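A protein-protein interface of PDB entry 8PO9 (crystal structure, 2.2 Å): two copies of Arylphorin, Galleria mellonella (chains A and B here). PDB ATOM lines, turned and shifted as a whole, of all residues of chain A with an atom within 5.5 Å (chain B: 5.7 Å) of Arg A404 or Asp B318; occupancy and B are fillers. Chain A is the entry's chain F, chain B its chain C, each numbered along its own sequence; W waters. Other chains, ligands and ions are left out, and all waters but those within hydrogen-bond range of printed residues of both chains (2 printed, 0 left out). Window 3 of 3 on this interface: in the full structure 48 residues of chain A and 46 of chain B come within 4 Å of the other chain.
Of the 12 printed residues of chain B, 3 touch a printed residue of chain A. Hydrophobic or aromatic side chains of chain B that line the printed part of chain A: Tyr B303. Along chain B the printed residues that touch a printed residue of chain A span positions 303 to 318. Hydrophobic or aromatic side chains of chain A that line the printed part of chain B: Tyr A320 and Pro A403. Among the printed residues, Asp or Glu carboxylates within 4 Å of a Lys or Arg side-chain nitrogen of the other chain: Arg A404 with Asp B318 (3.5 Å).
The side-chain hydroxyl (OH) of Tyr B303 sits at hydrogen-bond distance from the side-chain amide nitrogen (ND2) of Asn B317 (3.1 Å). The side-chain hydroxyl of Ser A324 is in hydrogen-bond range of the guanidinium group of Arg A404 (3.1 Å). The side-chain carboxylate (OD2) of Asp A326 lies within salt-bridge range of the guanidinium group (NH1) of Arg A404 (3.96 Å).
Arg A404 touches just one residue of chain B: Asp B318. Asp B318 touches one residue of chain A. Of the printed residues of chain B, Tyr A320 touches Asn B317 (3.5 Å). Of the printed residues of chain A, Asn B317 touches Tyr A320 (3.5 Å). Of the printed residues of chain A, Tyr B303 touches Pro A403 (3.7 Å). Of the printed residues of chain B, Pro A403 touches Tyr B303 (3.7 Å). Asp B319 touches none of the printed residues of chain A. Ser A406 touches none of the printed residues of chain B. The nearest residue of chain A that does not touch Asp B318 is Tyr A320 (4.4 Å). The nearest printed residue of chain B that does not touch Pro A403 is Ser B301 (6.3 Å).
1 position is printed for both chains. Of the 3 pairs that touch across the chains among the printed residues, none has its exchanged pair printed and touching as well.
The side-chain carboxylate of Asp B318 is in salt-bridge range of the guanidinium group of Arg A404.
Water W1 lies within hydrogen-bond range of the guanidinium group of Arg A404 (2.6 Å), the backbone carbonyl oxygen of Tyr A321 (2.9 Å) and the backbone carbonyl oxygen of Asp B318 (3.3 Å). Water W2 lies within hydrogen-bond range of the backbone carbonyl oxygen (O) of Asp B318, the backbone NH (N) of Tyr A321 and the backbone carbonyl oxygen (O) of Asp B319.
Tyr A320 touches Asn B317 (CD1 to OD1, 3.5 Å). Pro A403 touches Tyr B303.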
ATOM      1  N   TYR A 320      -9.377  20.705  24.733  1.00  0.00           N
ATOM      2  CA  TYR A 320      -9.954  20.152  23.514  1.00  0.00           C
ATOM      3  C   TYR A 320      -9.114  20.538  22.298  1.00  0.00           C
ATOM      4  O   TYR A 320      -8.791  21.711  22.098  1.00  0.00           O
ATOM      5  CB  TYR A 320     -11.388  20.664  23.369  1.00  0.00           C
ATOM      6  CG  TYR A 320     -12.076  20.278  22.089  1.00  0.00           C
ATOM      7  CD1 TYR A 320     -12.271  18.959  21.761  1.00  0.00           C
ATOM      8  CD2 TYR A 320     -12.513  21.252  21.194  1.00  0.00           C
ATOM      9  CE1 TYR A 320     -12.897  18.607  20.584  1.00  0.00           C
ATOM     10  CE2 TYR A 320     -13.152  20.911  20.010  1.00  0.00           C
ATOM     11  CZ  TYR A 320     -13.339  19.591  19.716  1.00  0.00           C
ATOM     12  OH  TYR A 320     -13.965  19.231  18.558  1.00  0.00           O
ATOM     13  N   TYR A 321      -8.787  19.551  21.469  1.00  0.00           N
ATOM     14  CA  TYR A 321      -7.933  19.750  20.299  1.00  0.00           C
ATOM     15  C   TYR A 321      -8.801  20.203  19.134  1.00  0.00           C
ATOM     16  O   TYR A 321      -9.623  19.434  18.621  1.00  0.00           O
ATOM     17  CB  TYR A 321      -7.188  18.459  19.962  1.00  0.00           C
ATOM     18  CG  TYR A 321      -6.249  18.554  18.775  1.00  0.00           C
ATOM     19  CD1 TYR A 321      -5.362  19.626  18.635  1.00  0.00           C
ATOM     20  CD2 TYR A 321      -6.237  17.559  17.799  1.00  0.00           C
ATOM     21  CE1 TYR A 321      -4.498  19.708  17.547  1.00  0.00           C
ATOM     22  CE2 TYR A 321      -5.379  17.632  16.711  1.00  0.00           C
ATOM     23  CZ  TYR A 321      -4.513  18.707  16.591  1.00  0.00           C
ATOM     24  OH  TYR A 321      -3.668  18.772  15.511  1.00  0.00           O
ATOM     25  N   LEU A 322      -8.597  21.441  18.692  1.00  0.00           N
ATOM     26  CA  LEU A 322      -9.481  22.017  17.689  1.00  0.00           C
ATOM     27  C   LEU A 322      -9.189  21.528  16.277  1.00  0.00           C
ATOM     28  O   LEU A 322     -10.087  21.555  15.431  1.00  0.00           O
ATOM     29  CB  LEU A 322      -9.382  23.540  17.724  1.00  0.00           C
ATOM     30  CG  LEU A 322      -9.581  24.235  19.068  1.00  0.00           C
ATOM     31  CD1 LEU A 322      -9.234  25.697  18.896  1.00  0.00           C
ATOM     32  CD2 LEU A 322     -11.027  24.067  19.579  1.00  0.00           C
ATOM     33  N   SER A 324      -8.504  18.668  14.415  1.00  0.00           N
ATOM     34  CA  SER A 324      -8.476  17.282  13.972  1.00  0.00           C
ATOM     35  C   SER A 324      -8.484  17.200  12.444  1.00  0.00           C
ATOM     36  O   SER A 324      -8.779  18.166  11.737  1.00  0.00           O
ATOM     37  CB  SER A 324      -9.691  16.531  14.485  1.00  0.00           C
ATOM     38  OG  SER A 324     -10.820  17.073  13.823  1.00  0.00           O
ATOM     39  N   ASP A 326     -10.704  15.735  10.832  1.00  0.00           N
ATOM     40  CA  ASP A 326     -12.079  16.053  10.451  1.00  0.00           C
ATOM     41  C   ASP A 326     -12.371  17.539  10.433  1.00  0.00           C
ATOM     42  O   ASP A 326     -13.391  17.933   9.871  1.00  0.00           O
ATOM     43  CB  ASP A 326     -13.054  15.359  11.380  1.00  0.00           C
ATOM     44  CG  ASP A 326     -13.101  13.883  11.145  1.00  0.00           C
ATOM     45  OD1 ASP A 326     -13.119  13.501   9.954  1.00  0.00           O
ATOM     46  OD2 ASP A 326     -13.054  13.115  12.128  1.00  0.00           O
ATOM     47  N   ASN A 327     -11.546  18.358  11.083  1.00  0.00           N
ATOM     48  CA  ASN A 327     -11.737  19.800  11.144  1.00  0.00           C
ATOM     49  C   ASN A 327     -10.837  20.572  10.197  1.00  0.00           C
ATOM     50  O   ASN A 327     -10.913  21.799  10.179  1.00  0.00           O
ATOM     51  CB  ASN A 327     -11.497  20.314  12.568  1.00  0.00           C
ATOM     52  CG  ASN A 327     -12.750  20.336  13.355  1.00  0.00           C
ATOM     53  OD1 ASN A 327     -13.778  19.874  12.869  1.00  0.00           O
ATOM     54  ND2 ASN A 327     -12.694  20.841  14.579  1.00  0.00           N
ATOM     55  N   ALA A 402     -19.106  20.224  18.989  1.00  0.00           N
ATOM     56  CA  ALA A 402     -20.086  19.231  18.584  1.00  0.00           C
ATOM     57  C   ALA A 402     -19.395  18.097  17.824  1.00  0.00           C
ATOM     58  O   ALA A 402     -18.359  18.309  17.192  1.00  0.00           O
ATOM     59  CB  ALA A 402     -21.160  19.874  17.708  1.00  0.00           C
ATOM     60  N   PRO A 403     -19.950  16.884  17.852  1.00  0.00           N
ATOM     61  CA  PRO A 403     -19.326  15.789  17.094  1.00  0.00           C
ATOM     62  C   PRO A 403     -19.239  16.121  15.608  1.00  0.00           C
ATOM     63  O   PRO A 403     -20.137  16.742  15.037  1.00  0.00           O
ATOM     64  CB  PRO A 403     -20.248  14.592  17.369  1.00  0.00           C
ATOM     65  CG  PRO A 403     -21.525  15.160  17.839  1.00  0.00           C
ATOM     66  CD  PRO A 403     -21.161  16.438  18.563  1.00  0.00           C
ATOM     67  N   ARG A 404     -18.140  15.688  14.981  1.00  0.00           N
ATOM     68  CA  ARG A 404     -17.875  16.067  13.592  1.00  0.00           C
ATOM     69  C   ARG A 404     -18.970  15.572  12.672  1.00  0.00           C
ATOM     70  O   ARG A 404     -19.287  16.228  11.673  1.00  0.00           O
ATOM     71  CB  ARG A 404     -16.529  15.509  13.109  1.00  0.00           C
ATOM     72  CG  ARG A 404     -15.316  16.251  13.664  1.00  0.00           C
ATOM     73  CD  ARG A 404     -15.130  15.945  15.140  1.00  0.00           C
ATOM     74  NE  ARG A 404     -13.985  16.610  15.766  1.00  0.00           N
ATOM     75  CZ  ARG A 404     -12.792  16.071  16.030  1.00  0.00           C
ATOM     76  NH1 ARG A 404     -12.478  14.826  15.653  1.00  0.00           N
ATOM     77  NH2 ARG A 404     -11.907  16.783  16.737  1.00  0.00           N
ATOM     78  N   SER A 405     -19.548  14.414  12.988  1.00  0.00           N
ATOM     79  CA  SER A 405     -20.709  13.931  12.251  1.00  0.00           C
ATOM     80  C   SER A 405     -21.870  14.914  12.313  1.00  0.00           C
ATOM     81  O   SER A 405     -22.690  14.965  11.389  1.00  0.00           O
ATOM     82  CB  SER A 405     -21.157  12.576  12.826  1.00  0.00           C
ATOM     83  OG  SER A 405     -21.465  12.695  14.212  1.00  0.00           O
ATOM     84  N   SER A 406     -21.975  15.684  13.404  1.00  0.00           N
ATOM     85  CA  SER A 406     -23.057  16.659  13.514  1.00  0.00           C
ATOM     86  C   SER A 406     -22.994  17.666  12.381  1.00  0.00           C
ATOM     87  O   SER A 406     -24.032  18.158  11.930  1.00  0.00           O
ATOM     88  CB  SER A 406     -22.999  17.363  14.882  1.00  0.00           C
ATOM     89  OG  SER A 406     -24.017  18.343  15.065  1.00  0.00           O
ATOM     90  N   ILE A 407     -21.801  17.915  11.856  1.00  0.00           N
ATOM     91  CA  ILE A 407     -21.641  18.857  10.761  1.00  0.00           C
ATOM     92  C   ILE A 407     -21.873  18.204   9.398  1.00  0.00           C
ATOM     93  O   ILE A 407     -22.384  18.857   8.481  1.00  0.00           O
ATOM     94  CB  ILE A 407     -20.239  19.480  10.854  1.00  0.00           C
ATOM     95  CG1 ILE A 407     -19.984  20.004  12.277  1.00  0.00           C
ATOM     96  CG2 ILE A 407     -20.056  20.582   9.807  1.00  0.00           C
ATOM     97  CD1 ILE A 407     -21.080  20.872  12.848  1.00  0.00           C
ATOM     98  N   ASN A 408     -21.532  16.921   9.249  1.00  0.00           N
ATOM     99  CA  ASN A 408     -21.623  16.269   7.942  1.00  0.00           C
ATOM    100  C   ASN A 408     -23.053  15.904   7.542  1.00  0.00           C
ATOM    101  O   ASN A 408     -23.345  15.831   6.343  1.00  0.00           O
ATOM    102  CB  ASN A 408     -20.705  15.046   7.913  1.00  0.00           C
ATOM    103  CG  ASN A 408     -19.253  15.433   8.188  1.00  0.00           C
ATOM    104  OD1 ASN A 408     -18.871  16.598   7.997  1.00  0.00           O
ATOM    105  ND2 ASN A 408     -18.431  14.463   8.587  1.00  0.00           N
ATOM    106  N   GLU B 219     -18.604   7.374  17.392  1.00  0.00           N
ATOM    107  CA  GLU B 219     -17.715   7.682  16.279  1.00  0.00           C
ATOM    108  C   GLU B 219     -17.119   6.390  15.733  1.00  0.00           C
ATOM    109  O   GLU B 219     -17.292   5.302  16.299  1.00  0.00           O
ATOM    110  CB  GLU B 219     -16.589   8.653  16.706  1.00  0.00           C
ATOM    111  CG  GLU B 219     -15.503   8.014  17.622  1.00  0.00           C
ATOM    112  CD  GLU B 219     -14.201   8.823  17.808  1.00  0.00           C
ATOM    113  OE1 GLU B 219     -13.625   9.418  16.875  1.00  0.00           O
ATOM    114  OE2 GLU B 219     -13.698   8.859  18.939  1.00  0.00           O
ATOM    115  N   ASP B 220     -16.343   6.541  14.650  1.00  0.00           N
ATOM    116  CA  ASP B 220     -15.572   5.447  14.047  1.00  0.00           C
ATOM    117  C   ASP B 220     -16.474   4.281  13.656  1.00  0.00           C
ATOM    118  O   ASP B 220     -16.134   3.112  13.844  1.00  0.00           O
ATOM    119  CB  ASP B 220     -14.429   4.996  14.970  1.00  0.00           C
ATOM    120  CG  ASP B 220     -13.369   6.092  15.149  1.00  0.00           C
ATOM    121  OD1 ASP B 220     -13.160   6.861  14.188  1.00  0.00           O
ATOM    122  OD2 ASP B 220     -12.744   6.196  16.231  1.00  0.00           O
ATOM    123  N   TYR B 298      -7.091  10.241  24.423  1.00  0.00           N
ATOM    124  CA  TYR B 298      -7.981   9.092  24.334  1.00  0.00           C
ATOM    125  C   TYR B 298      -8.814   9.210  23.053  1.00  0.00           C
ATOM    126  O   TYR B 298      -9.507  10.204  22.852  1.00  0.00           O
ATOM    127  CB  TYR B 298      -8.859   9.001  25.592  1.00  0.00           C
ATOM    128  CG  TYR B 298      -9.639   7.703  25.687  1.00  0.00           C
ATOM    129  CD1 TYR B 298      -8.992   6.482  25.948  1.00  0.00           C
ATOM    130  CD2 TYR B 298     -11.013   7.686  25.460  1.00  0.00           C
ATOM    131  CE1 TYR B 298      -9.708   5.284  26.013  1.00  0.00           C
ATOM    132  CE2 TYR B 298     -11.736   6.511  25.520  1.00  0.00           C
ATOM    133  CZ  TYR B 298     -11.075   5.310  25.785  1.00  0.00           C
ATOM    134  OH  TYR B 298     -11.809   4.168  25.833  1.00  0.00           O
ATOM    135  N   GLN B 299      -8.775   8.187  22.198  1.00  0.00           N
ATOM    136  CA  GLN B 299      -9.217   8.312  20.807  1.00  0.00           C
ATOM    137  C   GLN B 299     -10.648   7.841  20.546  1.00  0.00           C
ATOM    138  O   GLN B 299     -11.094   7.839  19.372  1.00  0.00           O
ATOM    139  CB  GLN B 299      -8.255   7.561  19.898  1.00  0.00           C
ATOM    140  CG  GLN B 299      -6.849   8.117  19.965  1.00  0.00           C
ATOM    141  CD  GLN B 299      -6.034   7.661  18.781  1.00  0.00           C
ATOM    142  OE1 GLN B 299      -6.086   8.281  17.730  1.00  0.00           O
ATOM    143  NE2 GLN B 299      -5.302   6.562  18.937  1.00  0.00           N
ATOM    144  N   THR B 300     -11.396   7.516  21.609  1.00  0.00           N
ATOM    145  CA  THR B 300     -12.773   7.038  21.508  1.00  0.00           C
ATOM    146  C   THR B 300     -13.709   8.035  22.197  1.00  0.00           C
ATOM    147  O   THR B 300     -13.909   7.977  23.419  1.00  0.00           O
ATOM    148  CB  THR B 300     -12.916   5.650  22.124  1.00  0.00           C
ATOM    149  OG1 THR B 300     -12.002   4.744  21.488  1.00  0.00           O
ATOM    150  CG2 THR B 300     -14.335   5.140  21.934  1.00  0.00           C
ATOM    151  N   SER B 301     -14.312   8.920  21.409  1.00  0.00           N
ATOM    152  CA  SER B 301     -15.249   9.898  21.936  1.00  0.00           C
ATOM    153  C   SER B 301     -16.597   9.238  22.254  1.00  0.00           C
ATOM    154  O   SER B 301     -16.882   8.106  21.851  1.00  0.00           O
ATOM    155  CB  SER B 301     -15.425  11.050  20.937  1.00  0.00           C
ATOM    156  OG  SER B 301     -15.981  10.595  19.717  1.00  0.00           O
ATOM    157  N   TYR B 303     -20.771  10.788  22.974  1.00  0.00           N
ATOM    158  CA  TYR B 303     -21.694  11.907  23.168  1.00  0.00           C
ATOM    159  C   TYR B 303     -23.058  11.319  23.499  1.00  0.00           C
ATOM    160  O   TYR B 303     -23.941  11.229  22.630  1.00  0.00           O
ATOM    161  CB  TYR B 303     -21.789  12.818  21.939  1.00  0.00           C
ATOM    162  CG  TYR B 303     -20.601  13.731  21.690  1.00  0.00           C
ATOM    163  CD1 TYR B 303     -19.495  13.282  20.981  1.00  0.00           C
ATOM    164  CD2 TYR B 303     -20.609  15.059  22.115  1.00  0.00           C
ATOM    165  CE1 TYR B 303     -18.408  14.116  20.737  1.00  0.00           C
ATOM    166  CE2 TYR B 303     -19.527  15.903  21.860  1.00  0.00           C
ATOM    167  CZ  TYR B 303     -18.446  15.420  21.179  1.00  0.00           C
ATOM    168  OH  TYR B 303     -17.383  16.229  20.927  1.00  0.00           O
ATOM    169  N   ARG B 316     -17.644  13.140  26.235  1.00  0.00           N
ATOM    170  CA  ARG B 316     -16.198  13.040  26.089  1.00  0.00           C
ATOM    171  C   ARG B 316     -15.863  13.350  24.635  1.00  0.00           C
ATOM    172  O   ARG B 316     -16.207  12.569  23.737  1.00  0.00           O
ATOM    173  CB  ARG B 316     -15.709  11.645  26.488  1.00  0.00           C
ATOM    174  CG  ARG B 316     -14.199  11.466  26.386  1.00  0.00           C
ATOM    175  CD  ARG B 316     -13.750  10.095  26.901  1.00  0.00           C
ATOM    176  NE  ARG B 316     -14.285   9.004  26.097  1.00  0.00           N
ATOM    177  CZ  ARG B 316     -15.168   8.088  26.482  1.00  0.00           C
ATOM    178  NH1 ARG B 316     -15.633   8.031  27.723  1.00  0.00           N
ATOM    179  NH2 ARG B 316     -15.578   7.183  25.603  1.00  0.00           N
ATOM    180  N   ASN B 317     -15.214  14.491  24.404  1.00  0.00           N
ATOM    181  CA  ASN B 317     -14.791  14.860  23.061  1.00  0.00           C
ATOM    182  C   ASN B 317     -13.725  13.881  22.582  1.00  0.00           C
ATOM    183  O   ASN B 317     -13.067  13.202  23.382  1.00  0.00           O
ATOM    184  CB  ASN B 317     -14.191  16.275  23.020  1.00  0.00           C
ATOM    185  CG  ASN B 317     -15.022  17.316  23.750  1.00  0.00           C
ATOM    186  OD1 ASN B 317     -14.453  18.219  24.364  1.00  0.00           O
ATOM    187  ND2 ASN B 317     -16.358  17.246  23.641  1.00  0.00           N
ATOM    188  N   ASP B 318     -13.537  13.831  21.260  1.00  0.00           N
ATOM    189  CA  ASP B 318     -12.475  13.003  20.696  1.00  0.00           C
ATOM    190  C   ASP B 318     -11.114  13.515  21.169  1.00  0.00           C
ATOM    191  O   ASP B 318     -10.901  14.725  21.322  1.00  0.00           O
ATOM    192  CB  ASP B 318     -12.540  13.020  19.168  1.00  0.00           C
ATOM    193  CG  ASP B 318     -12.000  11.735  18.518  1.00  0.00           C
ATOM    194  OD1 ASP B 318     -11.804  10.665  19.176  1.00  0.00           O
ATOM    195  OD2 ASP B 318     -11.772  11.803  17.297  1.00  0.00           O
ATOM    196  N   ASP B 319     -10.179  12.578  21.379  1.00  0.00           N
ATOM    197  CA  ASP B 319      -8.809  12.912  21.785  1.00  0.00           C
ATOM    198  C   ASP B 319      -8.747  13.629  23.129  1.00  0.00           C
ATOM    199  O   ASP B 319      -7.857  14.445  23.367  1.00  0.00           O
ATOM    200  CB  ASP B 319      -8.105  13.731  20.704  1.00  0.00           C
ATOM    201  CG  ASP B 319      -7.806  12.906  19.479  1.00  0.00           C
ATOM    202  OD1 ASP B 319      -7.717  11.668  19.623  1.00  0.00           O
ATOM    203  OD2 ASP B 319      -7.686  13.480  18.379  1.00  0.00           O
ATOM    204  N   TYR B 320      -9.660  13.291  24.030  1.00  0.00           N
ATOM    205  CA  TYR B 320      -9.654  13.870  25.366  1.00  0.00           C
ATOM    206  C   TYR B 320      -8.383  13.476  26.119  1.00  0.00           C
ATOM    207  O   TYR B 320      -7.982  12.307  26.130  1.00  0.00           O
ATOM    208  CB  TYR B 320     -10.898  13.409  26.122  1.00  0.00           C
ATOM    209  CG  TYR B 320     -10.992  13.871  27.560  1.00  0.00           C
ATOM    210  CD1 TYR B 320     -10.978  15.223  27.888  1.00  0.00           C
ATOM    211  CD2 TYR B 320     -11.162  12.959  28.587  1.00  0.00           C
ATOM    212  CE1 TYR B 320     -11.099  15.651  29.218  1.00  0.00           C
ATOM    213  CE2 TYR B 320     -11.269  13.371  29.908  1.00  0.00           C
ATOM    214  CZ  TYR B 320     -11.243  14.718  30.218  1.00  0.00           C
ATOM    215  OH  TYR B 320     -11.358  15.103  31.546  1.00  0.00           O
HETATM  216  O   HOH W   1     -10.155  16.627  18.695  1.00  0.00           O
HETATM  217  O   HOH W   2      -9.310  16.837  22.385  1.00  0.00           O
